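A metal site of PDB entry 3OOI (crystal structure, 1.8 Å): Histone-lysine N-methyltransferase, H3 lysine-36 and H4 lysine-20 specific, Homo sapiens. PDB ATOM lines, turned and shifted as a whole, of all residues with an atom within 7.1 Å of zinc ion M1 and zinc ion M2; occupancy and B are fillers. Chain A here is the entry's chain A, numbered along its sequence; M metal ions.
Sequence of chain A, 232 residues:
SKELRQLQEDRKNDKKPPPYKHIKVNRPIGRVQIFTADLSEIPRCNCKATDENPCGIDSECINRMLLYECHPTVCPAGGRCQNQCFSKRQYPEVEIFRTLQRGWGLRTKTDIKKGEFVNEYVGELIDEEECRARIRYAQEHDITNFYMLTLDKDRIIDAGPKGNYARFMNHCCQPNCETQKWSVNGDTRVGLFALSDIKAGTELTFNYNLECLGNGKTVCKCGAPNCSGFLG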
ATOM      1  N   ARG A  44      17.647 -30.222   1.287  1.00  0.00           N
ATOM      2  CA  ARG A  44      17.879 -30.860  -0.004  1.00  0.00           C
ATOM      3  C   ARG A  44      16.608 -30.644  -0.808  1.00  0.00           C
ATOM      4  O   ARG A  44      15.519 -30.968  -0.330  1.00  0.00           O
ATOM      5  CB  ARG A  44      18.113 -32.360   0.156  1.00  0.00           C
ATOM      6  CG  ARG A  44      19.465 -32.762   0.765  1.00  0.00           C
ATOM      7  CD  ARG A  44      19.504 -34.284   0.937  1.00  0.00           C
ATOM      8  NE  ARG A  44      20.832 -34.807   1.286  1.00  0.00           N
ATOM      9  CZ  ARG A  44      21.274 -34.934   2.532  1.00  0.00           C
ATOM     10  NH1 ARG A  44      20.513 -34.553   3.555  1.00  0.00           N
ATOM     11  NH2 ARG A  44      22.486 -35.438   2.764  1.00  0.00           N
ATOM     12  N   CYS A  45      16.743 -30.098  -2.009  1.00  0.00           N
ATOM     13  CA  CYS A  45      15.592 -29.843  -2.882  1.00  0.00           C
ATOM     14  C   CYS A  45      15.141 -31.080  -3.660  1.00  0.00           C
ATOM     15  O   CYS A  45      15.692 -32.183  -3.530  1.00  0.00           O
ATOM     16  CB  CYS A  45      15.917 -28.719  -3.862  1.00  0.00           C
ATOM     17  SG  CYS A  45      17.098 -29.262  -5.152  1.00  0.00           S
ATOM     18  N   ASN A  46      14.099 -30.868  -4.467  1.00  0.00           N
ATOM     19  CA  ASN A  46      13.442 -31.891  -5.282  1.00  0.00           C
ATOM     20  C   ASN A  46      14.045 -32.051  -6.678  1.00  0.00           C
ATOM     21  O   ASN A  46      13.580 -32.879  -7.450  1.00  0.00           O
ATOM     22  CB  ASN A  46      11.933 -31.573  -5.385  1.00  0.00           C
ATOM     23  CG  ASN A  46      11.659 -30.137  -5.826  1.00  0.00           C
ATOM     24  OD1 ASN A  46      12.292 -29.177  -5.335  1.00  0.00           O
ATOM     25  ND2 ASN A  46      10.714 -29.961  -6.765  1.00  0.00           N
ATOM     26  N   CYS A  47      15.081 -31.280  -7.002  1.00  0.00           N
ATOM     27  CA  CYS A  47      15.678 -31.353  -8.344  1.00  0.00           C
ATOM     28  C   CYS A  47      16.566 -32.575  -8.518  1.00  0.00           C
ATOM     29  O   CYS A  47      17.129 -33.091  -7.543  1.00  0.00           O
ATOM     30  CB  CYS A  47      16.471 -30.092  -8.698  1.00  0.00           C
ATOM     31  SG  CYS A  47      15.484 -28.579  -8.592  1.00  0.00           S
ATOM     32  N   LYS A  48      16.691 -33.014  -9.763  1.00  0.00           N
ATOM     33  CA  LYS A  48      17.524 -34.160 -10.083  1.00  0.00           C
ATOM     34  C   LYS A  48      18.588 -33.714 -11.074  1.00  0.00           C
ATOM     35  O   LYS A  48      18.367 -32.770 -11.849  1.00  0.00           O
ATOM     36  CB  LYS A  48      16.681 -35.304 -10.662  1.00  0.00           C
ATOM     37  CG  LYS A  48      15.557 -35.842  -9.737  1.00  0.00           C
ATOM     38  CD  LYS A  48      16.065 -36.248  -8.344  1.00  0.00           C
ATOM     39  CE  LYS A  48      14.944 -36.791  -7.447  1.00  0.00           C
ATOM     40  NZ  LYS A  48      14.001 -35.763  -6.933  1.00  0.00           N
ATOM     41  N   ASP A  51      17.595 -33.217 -14.747  1.00  0.00           N
ATOM     42  CA  ASP A  51      16.646 -32.185 -15.142  1.00  0.00           C
ATOM     43  C   ASP A  51      17.318 -31.222 -16.109  1.00  0.00           C
ATOM     44  O   ASP A  51      18.547 -31.116 -16.109  1.00  0.00           O
ATOM     45  CB  ASP A  51      16.100 -31.415 -13.937  1.00  0.00           C
ATOM     46  CG  ASP A  51      15.235 -32.288 -13.009  1.00  0.00           C
ATOM     47  OD1 ASP A  51      14.792 -33.395 -13.416  1.00  0.00           O
ATOM     48  OD2 ASP A  51      14.986 -31.851 -11.869  1.00  0.00           O
ATOM     49  N   ASN A  53      17.517 -27.837 -16.306  1.00  0.00           N
ATOM     50  CA  ASN A  53      18.245 -26.745 -15.659  1.00  0.00           C
ATOM     51  C   ASN A  53      18.021 -26.836 -14.167  1.00  0.00           C
ATOM     52  O   ASN A  53      17.213 -26.076 -13.610  1.00  0.00           O
ATOM     53  CB  ASN A  53      17.769 -25.376 -16.181  1.00  0.00           C
ATOM     54  CG  ASN A  53      18.296 -25.053 -17.571  1.00  0.00           C
ATOM     55  OD1 ASN A  53      19.487 -24.762 -17.751  1.00  0.00           O
ATOM     56  ND2 ASN A  53      17.412 -25.095 -18.569  1.00  0.00           N
ATOM     57  N   PRO A  54      18.704 -27.786 -13.503  1.00  0.00           N
ATOM     58  CA  PRO A  54      18.445 -28.096 -12.097  1.00  0.00           C
ATOM     59  C   PRO A  54      18.599 -26.860 -11.205  1.00  0.00           C
ATOM     60  O   PRO A  54      19.613 -26.148 -11.301  1.00  0.00           O
ATOM     61  CB  PRO A  54      19.523 -29.139 -11.754  1.00  0.00           C
ATOM     62  CG  PRO A  54      20.019 -29.664 -13.062  1.00  0.00           C
ATOM     63  CD  PRO A  54      19.865 -28.544 -14.034  1.00  0.00           C
ATOM     64  N   CYS A  55      17.580 -26.617 -10.391  1.00  0.00           N
ATOM     65  CA  CYS A  55      17.532 -25.500  -9.436  1.00  0.00           C
ATOM     66  C   CYS A  55      17.589 -24.142 -10.134  1.00  0.00           C
ATOM     67  O   CYS A  55      17.863 -23.135  -9.493  1.00  0.00           O
ATOM     68  CB  CYS A  55      18.636 -25.638  -8.366  1.00  0.00           C
ATOM     69  SG  CYS A  55      18.852 -27.337  -7.749  1.00  0.00           S
ATOM     70  N   GLY A  56      17.285 -24.130 -11.428  1.00  0.00           N
ATOM     71  CA  GLY A  56      17.299 -22.895 -12.205  1.00  0.00           C
ATOM     72  C   GLY A  56      16.053 -22.065 -11.996  1.00  0.00           C
ATOM     73  O   GLY A  56      15.083 -22.523 -11.362  1.00  0.00           O
ATOM     74  N   SER A  59      12.841 -23.720 -12.927  1.00  0.00           N
ATOM     75  CA  SER A  59      12.686 -25.116 -12.464  1.00  0.00           C
ATOM     76  C   SER A  59      11.665 -25.243 -11.341  1.00  0.00           C
ATOM     77  O   SER A  59      11.175 -24.245 -10.834  1.00  0.00           O
ATOM     78  CB  SER A  59      14.028 -25.648 -11.948  1.00  0.00           C
ATOM     79  OG  SER A  59      14.322 -25.054 -10.699  1.00  0.00           O
ATOM     80  N   GLU A  60      11.396 -26.476 -10.935  1.00  0.00           N
ATOM     81  CA  GLU A  60      10.423 -26.757  -9.870  1.00  0.00           C
ATOM     82  C   GLU A  60      11.056 -26.664  -8.477  1.00  0.00           C
ATOM     83  O   GLU A  60      10.448 -27.063  -7.481  1.00  0.00           O
ATOM     84  CB  GLU A  60       9.813 -28.159 -10.061  1.00  0.00           C
ATOM     85  CG  GLU A  60       9.096 -28.390 -11.413  1.00  0.00           C
ATOM     86  CD  GLU A  60       8.755 -29.866 -11.694  1.00  0.00           C
ATOM     87  OE1 GLU A  60       8.207 -30.146 -12.777  1.00  0.00           O
ATOM     88  OE2 GLU A  60       9.034 -30.751 -10.841  1.00  0.00           O
ATOM     89  N   CYS A  61      12.289 -26.160  -8.410  1.00  0.00           N
ATOM     90  CA  CYS A  61      13.107 -26.234  -7.198  1.00  0.00           C
ATOM     91  C   CYS A  61      12.453 -25.603  -5.961  1.00  0.00           C
ATOM     92  O   CYS A  61      12.176 -24.406  -5.964  1.00  0.00           O
ATOM     93  CB  CYS A  61      14.449 -25.545  -7.434  1.00  0.00           C
ATOM     94  SG  CYS A  61      15.656 -25.707  -6.079  1.00  0.00           S
ATOM     95  N   ILE A  62      12.258 -26.406  -4.925  1.00  0.00           N
ATOM     96  CA  ILE A  62      11.674 -25.931  -3.661  1.00  0.00           C
ATOM     97  C   ILE A  62      12.607 -25.020  -2.884  1.00  0.00           C
ATOM     98  O   ILE A  62      12.138 -24.140  -2.148  1.00  0.00           O
ATOM     99  CB  ILE A  62      11.188 -27.126  -2.783  1.00  0.00           C
ATOM    100  CG1 ILE A  62      10.279 -26.645  -1.635  1.00  0.00           C
ATOM    101  CG2 ILE A  62      12.367 -27.943  -2.261  1.00  0.00           C
ATOM    102  CD1 ILE A  62       9.059 -25.819  -2.072  1.00  0.00           C
ATOM    103  N   ASN A  63      13.924 -25.233  -2.983  1.00  0.00           N
ATOM    104  CA  ASN A  63      14.856 -24.350  -2.252  1.00  0.00           C
ATOM    105  C   ASN A  63      14.736 -22.950  -2.841  1.00  0.00           C
ATOM    106  O   ASN A  63      14.529 -21.967  -2.111  1.00  0.00           O
ATOM    107  CB  ASN A  63      16.316 -24.864  -2.350  1.00  0.00           C
ATOM    108  CG  ASN A  63      16.624 -25.983  -1.334  1.00  0.00           C
ATOM    109  OD1 ASN A  63      17.775 -26.459  -1.264  1.00  0.00           O
ATOM    110  ND2 ASN A  63      15.636 -26.402  -0.559  1.00  0.00           N
ATOM    111  N   ARG A  64      14.833 -22.860  -4.159  1.00  0.00           N
ATOM    112  CA  ARG A  64      14.653 -21.588  -4.831  1.00  0.00           C
ATOM    113  C   ARG A  64      13.286 -20.954  -4.509  1.00  0.00           C
ATOM    114  O   ARG A  64      13.207 -19.764  -4.222  1.00  0.00           O
ATOM    115  CB  ARG A  64      14.836 -21.759  -6.345  1.00  0.00           C
ATOM    116  CG  ARG A  64      14.499 -20.518  -7.142  1.00  0.00           C
ATOM    117  CD  ARG A  64      14.809 -20.720  -8.628  1.00  0.00           C
ATOM    118  NE  ARG A  64      16.252 -20.809  -8.916  1.00  0.00           N
ATOM    119  CZ  ARG A  64      17.073 -19.765  -8.991  1.00  0.00           C
ATOM    120  NH1 ARG A  64      16.637 -18.524  -8.753  1.00  0.00           N
ATOM    121  NH2 ARG A  64      18.352 -19.970  -9.284  1.00  0.00           N
ATOM    122  N   GLU A  69      19.303 -20.846  -0.596  1.00  0.00           N
ATOM    123  CA  GLU A  69      20.356 -21.192  -1.518  1.00  0.00           C
ATOM    124  C   GLU A  69      20.790 -22.643  -1.272  1.00  0.00           C
ATOM    125  O   GLU A  69      20.842 -23.092  -0.116  1.00  0.00           O
ATOM    126  CB  GLU A  69      21.526 -20.219  -1.359  1.00  0.00           C
ATOM    127  CG  GLU A  69      22.664 -20.522  -2.278  1.00  0.00           C
ATOM    128  CD  GLU A  69      23.452 -19.293  -2.638  1.00  0.00           C
ATOM    129  OE1 GLU A  69      24.662 -19.321  -2.429  1.00  0.00           O
ATOM    130  OE2 GLU A  69      22.856 -18.329  -3.153  1.00  0.00           O
ATOM    131  N   CYS A  70      21.027 -23.412  -2.345  1.00  0.00           N
ATOM    132  CA  CYS A  70      21.548 -24.775  -2.192  1.00  0.00           C
ATOM    133  C   CYS A  70      23.017 -24.726  -1.757  1.00  0.00           C
ATOM    134  O   CYS A  70      23.711 -23.749  -2.036  1.00  0.00           O
ATOM    135  CB  CYS A  70      21.475 -25.556  -3.516  1.00  0.00           C
ATOM    136  SG  CYS A  70      19.778 -25.852  -4.153  1.00  0.00           S
ATOM    137  N   HIS A  71      23.463 -25.763  -1.066  1.00  0.00           N
ATOM    138  CA  HIS A  71      24.904 -25.941  -0.793  1.00  0.00           C
ATOM    139  C   HIS A  71      25.506 -26.944  -1.792  1.00  0.00           C
ATOM    140  O   HIS A  71      24.928 -28.001  -2.023  1.00  0.00           O
ATOM    141  CB  HIS A  71      25.109 -26.401   0.633  1.00  0.00           C
ATOM    142  CG  HIS A  71      26.551 -26.387   1.053  1.00  0.00           C
ATOM    143  ND1 HIS A  71      27.094 -25.362   1.791  1.00  0.00           N
ATOM    144  CD2 HIS A  71      27.560 -27.229   0.767  1.00  0.00           C
ATOM    145  CE1 HIS A  71      28.384 -25.593   1.967  1.00  0.00           C
ATOM    146  NE2 HIS A  71      28.692 -26.716   1.353  1.00  0.00           N
ATOM    147  N   VAL A  74      25.769 -30.660  -0.887  1.00  0.00           N
ATOM    148  CA  VAL A  74      24.492 -31.262  -0.441  1.00  0.00           C
ATOM    149  C   VAL A  74      23.461 -31.413  -1.578  1.00  0.00           C
ATOM    150  O   VAL A  74      22.708 -32.399  -1.619  1.00  0.00           O
ATOM    151  CB  VAL A  74      23.908 -30.413   0.717  1.00  0.00           C
ATOM    152  CG1 VAL A  74      22.516 -30.903   1.157  1.00  0.00           C
ATOM    153  CG2 VAL A  74      24.866 -30.443   1.917  1.00  0.00           C
ATOM    154  N   CYS A  75      23.435 -30.448  -2.505  1.00  0.00           N
ATOM    155  CA  CYS A  75      22.370 -30.451  -3.509  1.00  0.00           C
ATOM    156  C   CYS A  75      22.323 -31.762  -4.308  1.00  0.00           C
ATOM    157  O   CYS A  75      23.351 -32.240  -4.794  1.00  0.00           O
ATOM    158  CB  CYS A  75      22.507 -29.284  -4.484  1.00  0.00           C
ATOM    159  SG  CYS A  75      21.115 -29.264  -5.644  1.00  0.00           S
ATOM    160  N   PRO A  76      21.123 -32.365  -4.437  1.00  0.00           N
ATOM    161  CA  PRO A  76      21.013 -33.577  -5.269  1.00  0.00           C
ATOM    162  C   PRO A  76      21.422 -33.409  -6.724  1.00  0.00           C
ATOM    163  O   PRO A  76      21.757 -34.396  -7.380  1.00  0.00           O
ATOM    164  CB  PRO A  76      19.521 -33.931  -5.166  1.00  0.00           C
ATOM    165  CG  PRO A  76      19.141 -33.444  -3.799  1.00  0.00           C
ATOM    166  CD  PRO A  76      19.871 -32.110  -3.683  1.00  0.00           C
ATOM    167  N   ALA A  77      21.395 -32.181  -7.237  1.00  0.00           N
ATOM    168  CA  ALA A  77      21.779 -31.911  -8.620  1.00  0.00           C
ATOM    169  C   ALA A  77      23.310 -31.768  -8.803  1.00  0.00           C
ATOM    170  O   ALA A  77      23.799 -31.597  -9.936  1.00  0.00           O
ATOM    171  CB  ALA A  77      21.058 -30.677  -9.150  1.00  0.00           C
ATOM    172  N   GLY A  78      24.040 -31.835  -7.699  1.00  0.00           N
ATOM    173  CA  GLY A  78      25.509 -31.688  -7.715  1.00  0.00           C
ATOM    174  C   GLY A  78      25.955 -30.427  -8.415  1.00  0.00           C
ATOM    175  O   GLY A  78      25.350 -29.354  -8.244  1.00  0.00           O
ATOM    176  N   ARG A  80      25.535 -29.464 -11.289  1.00  0.00           N
ATOM    177  CA  ARG A  80      24.553 -28.898 -12.208  1.00  0.00           C
ATOM    178  C   ARG A  80      23.597 -27.905 -11.554  1.00  0.00           C
ATOM    179  O   ARG A  80      22.836 -27.226 -12.237  1.00  0.00           O
ATOM    180  CB  ARG A  80      23.807 -30.016 -12.935  1.00  0.00           C
ATOM    181  CG  ARG A  80      24.784 -31.040 -13.568  1.00  0.00           C
ATOM    182  CD  ARG A  80      24.450 -31.419 -14.985  1.00  0.00           C
ATOM    183  NE  ARG A  80      23.043 -31.705 -15.208  1.00  0.00           N
ATOM    184  CZ  ARG A  80      22.254 -30.993 -16.016  1.00  0.00           C
ATOM    185  NH1 ARG A  80      22.731 -29.966 -16.692  1.00  0.00           N
ATOM    186  NH2 ARG A  80      20.977 -31.328 -16.153  1.00  0.00           N
ATOM    187  N   CYS A  81      23.659 -27.814 -10.220  1.00  0.00           N
ATOM    188  CA  CYS A  81      22.812 -26.897  -9.437  1.00  0.00           C
ATOM    189  C   CYS A  81      22.982 -25.449  -9.890  1.00  0.00           C
ATOM    190  O   CYS A  81      24.112 -24.945  -9.935  1.00  0.00           O
ATOM    191  CB  CYS A  81      23.136 -27.017  -7.943  1.00  0.00           C
ATOM    192  SG  CYS A  81      22.307 -25.798  -6.893  1.00  0.00           S
ATOM    193  N   GLN A  82      21.868 -24.784 -10.199  1.00  0.00           N
ATOM    194  CA  GLN A  82      21.873 -23.391 -10.654  1.00  0.00           C
ATOM    195  C   GLN A  82      21.336 -22.441  -9.581  1.00  0.00           C
ATOM    196  O   GLN A  82      20.907 -21.324  -9.884  1.00  0.00           O
ATOM    197  CB  GLN A  82      21.085 -23.246 -11.955  1.00  0.00           C
ATOM    198  CG  GLN A  82      21.675 -24.046 -13.113  1.00  0.00           C
ATOM    199  CD  GLN A  82      20.892 -23.861 -14.402  1.00  0.00           C
ATOM    200  OE1 GLN A  82      20.062 -22.955 -14.514  1.00  0.00           O
ATOM    201  NE2 GLN A  82      21.161 -24.729 -15.381  1.00  0.00           N
ATOM    202  N   ASN A  83      21.385 -22.874  -8.326  1.00  0.00           N
ATOM    203  CA  ASN A  83      20.841 -22.076  -7.213  1.00  0.00           C
ATOM    204  C   ASN A  83      21.902 -21.731  -6.163  1.00  0.00           C
ATOM    205  O   ASN A  83      21.741 -22.011  -4.981  1.00  0.00           O
ATOM    206  CB  ASN A  83      19.663 -22.829  -6.580  1.00  0.00           C
ATOM    207  CG  ASN A  83      18.938 -22.029  -5.492  1.00  0.00           C
ATOM    208  OD1 ASN A  83      18.828 -20.803  -5.579  1.00  0.00           O
ATOM    209  ND2 ASN A  83      18.449 -22.710  -4.463  1.00  0.00           N
ATOM    210  N   GLN A  84      22.999 -21.128  -6.616  1.00  0.00           N
ATOM    211  CA  GLN A  84      24.086 -20.704  -5.702  1.00  0.00           C
ATOM    212  C   GLN A  84      24.493 -19.269  -6.042  1.00  0.00           C
ATOM    213  O   GLN A  84      25.673 -18.931  -6.024  1.00  0.00           O
ATOM    214  CB  GLN A  84      25.269 -21.674  -5.785  1.00  0.00           C
ATOM    215  CG  GLN A  84      24.919 -23.079  -5.257  1.00  0.00           C
ATOM    216  CD  GLN A  84      25.944 -24.141  -5.623  1.00  0.00           C
ATOM    217  OE1 GLN A  84      27.154 -23.888  -5.631  1.00  0.00           O
ATOM    218  NE2 GLN A  84      25.463 -25.353  -5.905  1.00  0.00           N
HETATM  219 ZN    ZN M   1      20.489 -27.049  -6.039  1.00  0.00          ZN
HETATM  220 ZN    ZN M   2      16.752 -27.662  -6.744  1.00  0.00          ZN
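The side-chain sulfur (SG) of Cys 75 sits close to the backbone NH (N) of Ala 77, at 3.3 Å. The side-chain sulfur (SG) of Cys 61 lies close to the backbone NH (N) of Asn 63 (3.6 Å). N of Cys 61 sits close to OG of Ser 59 (3.3 Å). The side-chain sulfur (SG) of Cys 61 lies close to the backbone NH (N) of Arg 64, at 3.5 Å. N of Cys 70 sits at hydrogen-bond distance from O of Asn 83, at 3.1 Å. OD1 of Asn 63 sits close to SG of Cys 70, at 3.6 Å. SG of Cys 81 sits close to N of Asn 83, at 3.4 Å. The side-chain sulfur of Cys 81 sits close to the side-chain amide nitrogen of Gln 84, 3.3 Å away.
Zinc ion M1 is bound by the side-chain sulfur (SG) of Cys 75 (2.3 Å), the side-chain sulfur (SG) of Cys 70 (2.3 Å), the side-chain sulfur (SG) of Cys 81 (2.4 Å) and the side-chain sulfur (SG) of Cys 55 (2.4 Å). Zinc ion M1 has four donor atoms within binding distance.
Four residues have an atom within 4 Å of zinc ion M1: Cys 55, Cys 70, Cys 75 and Cys 81.
Zinc ion M2 is bound by the side-chain sulfur of Cys 45 (2.3 Å), the side-chain sulfur of Cys 61 (2.3 Å), the side-chain sulfur of Cys 55 (2.4 Å) and the side-chain sulfur of Cys 47 (2.4 Å).
The nearest printed residue that does not touch zinc ion M2 is Cys 70 (4.4 Å).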
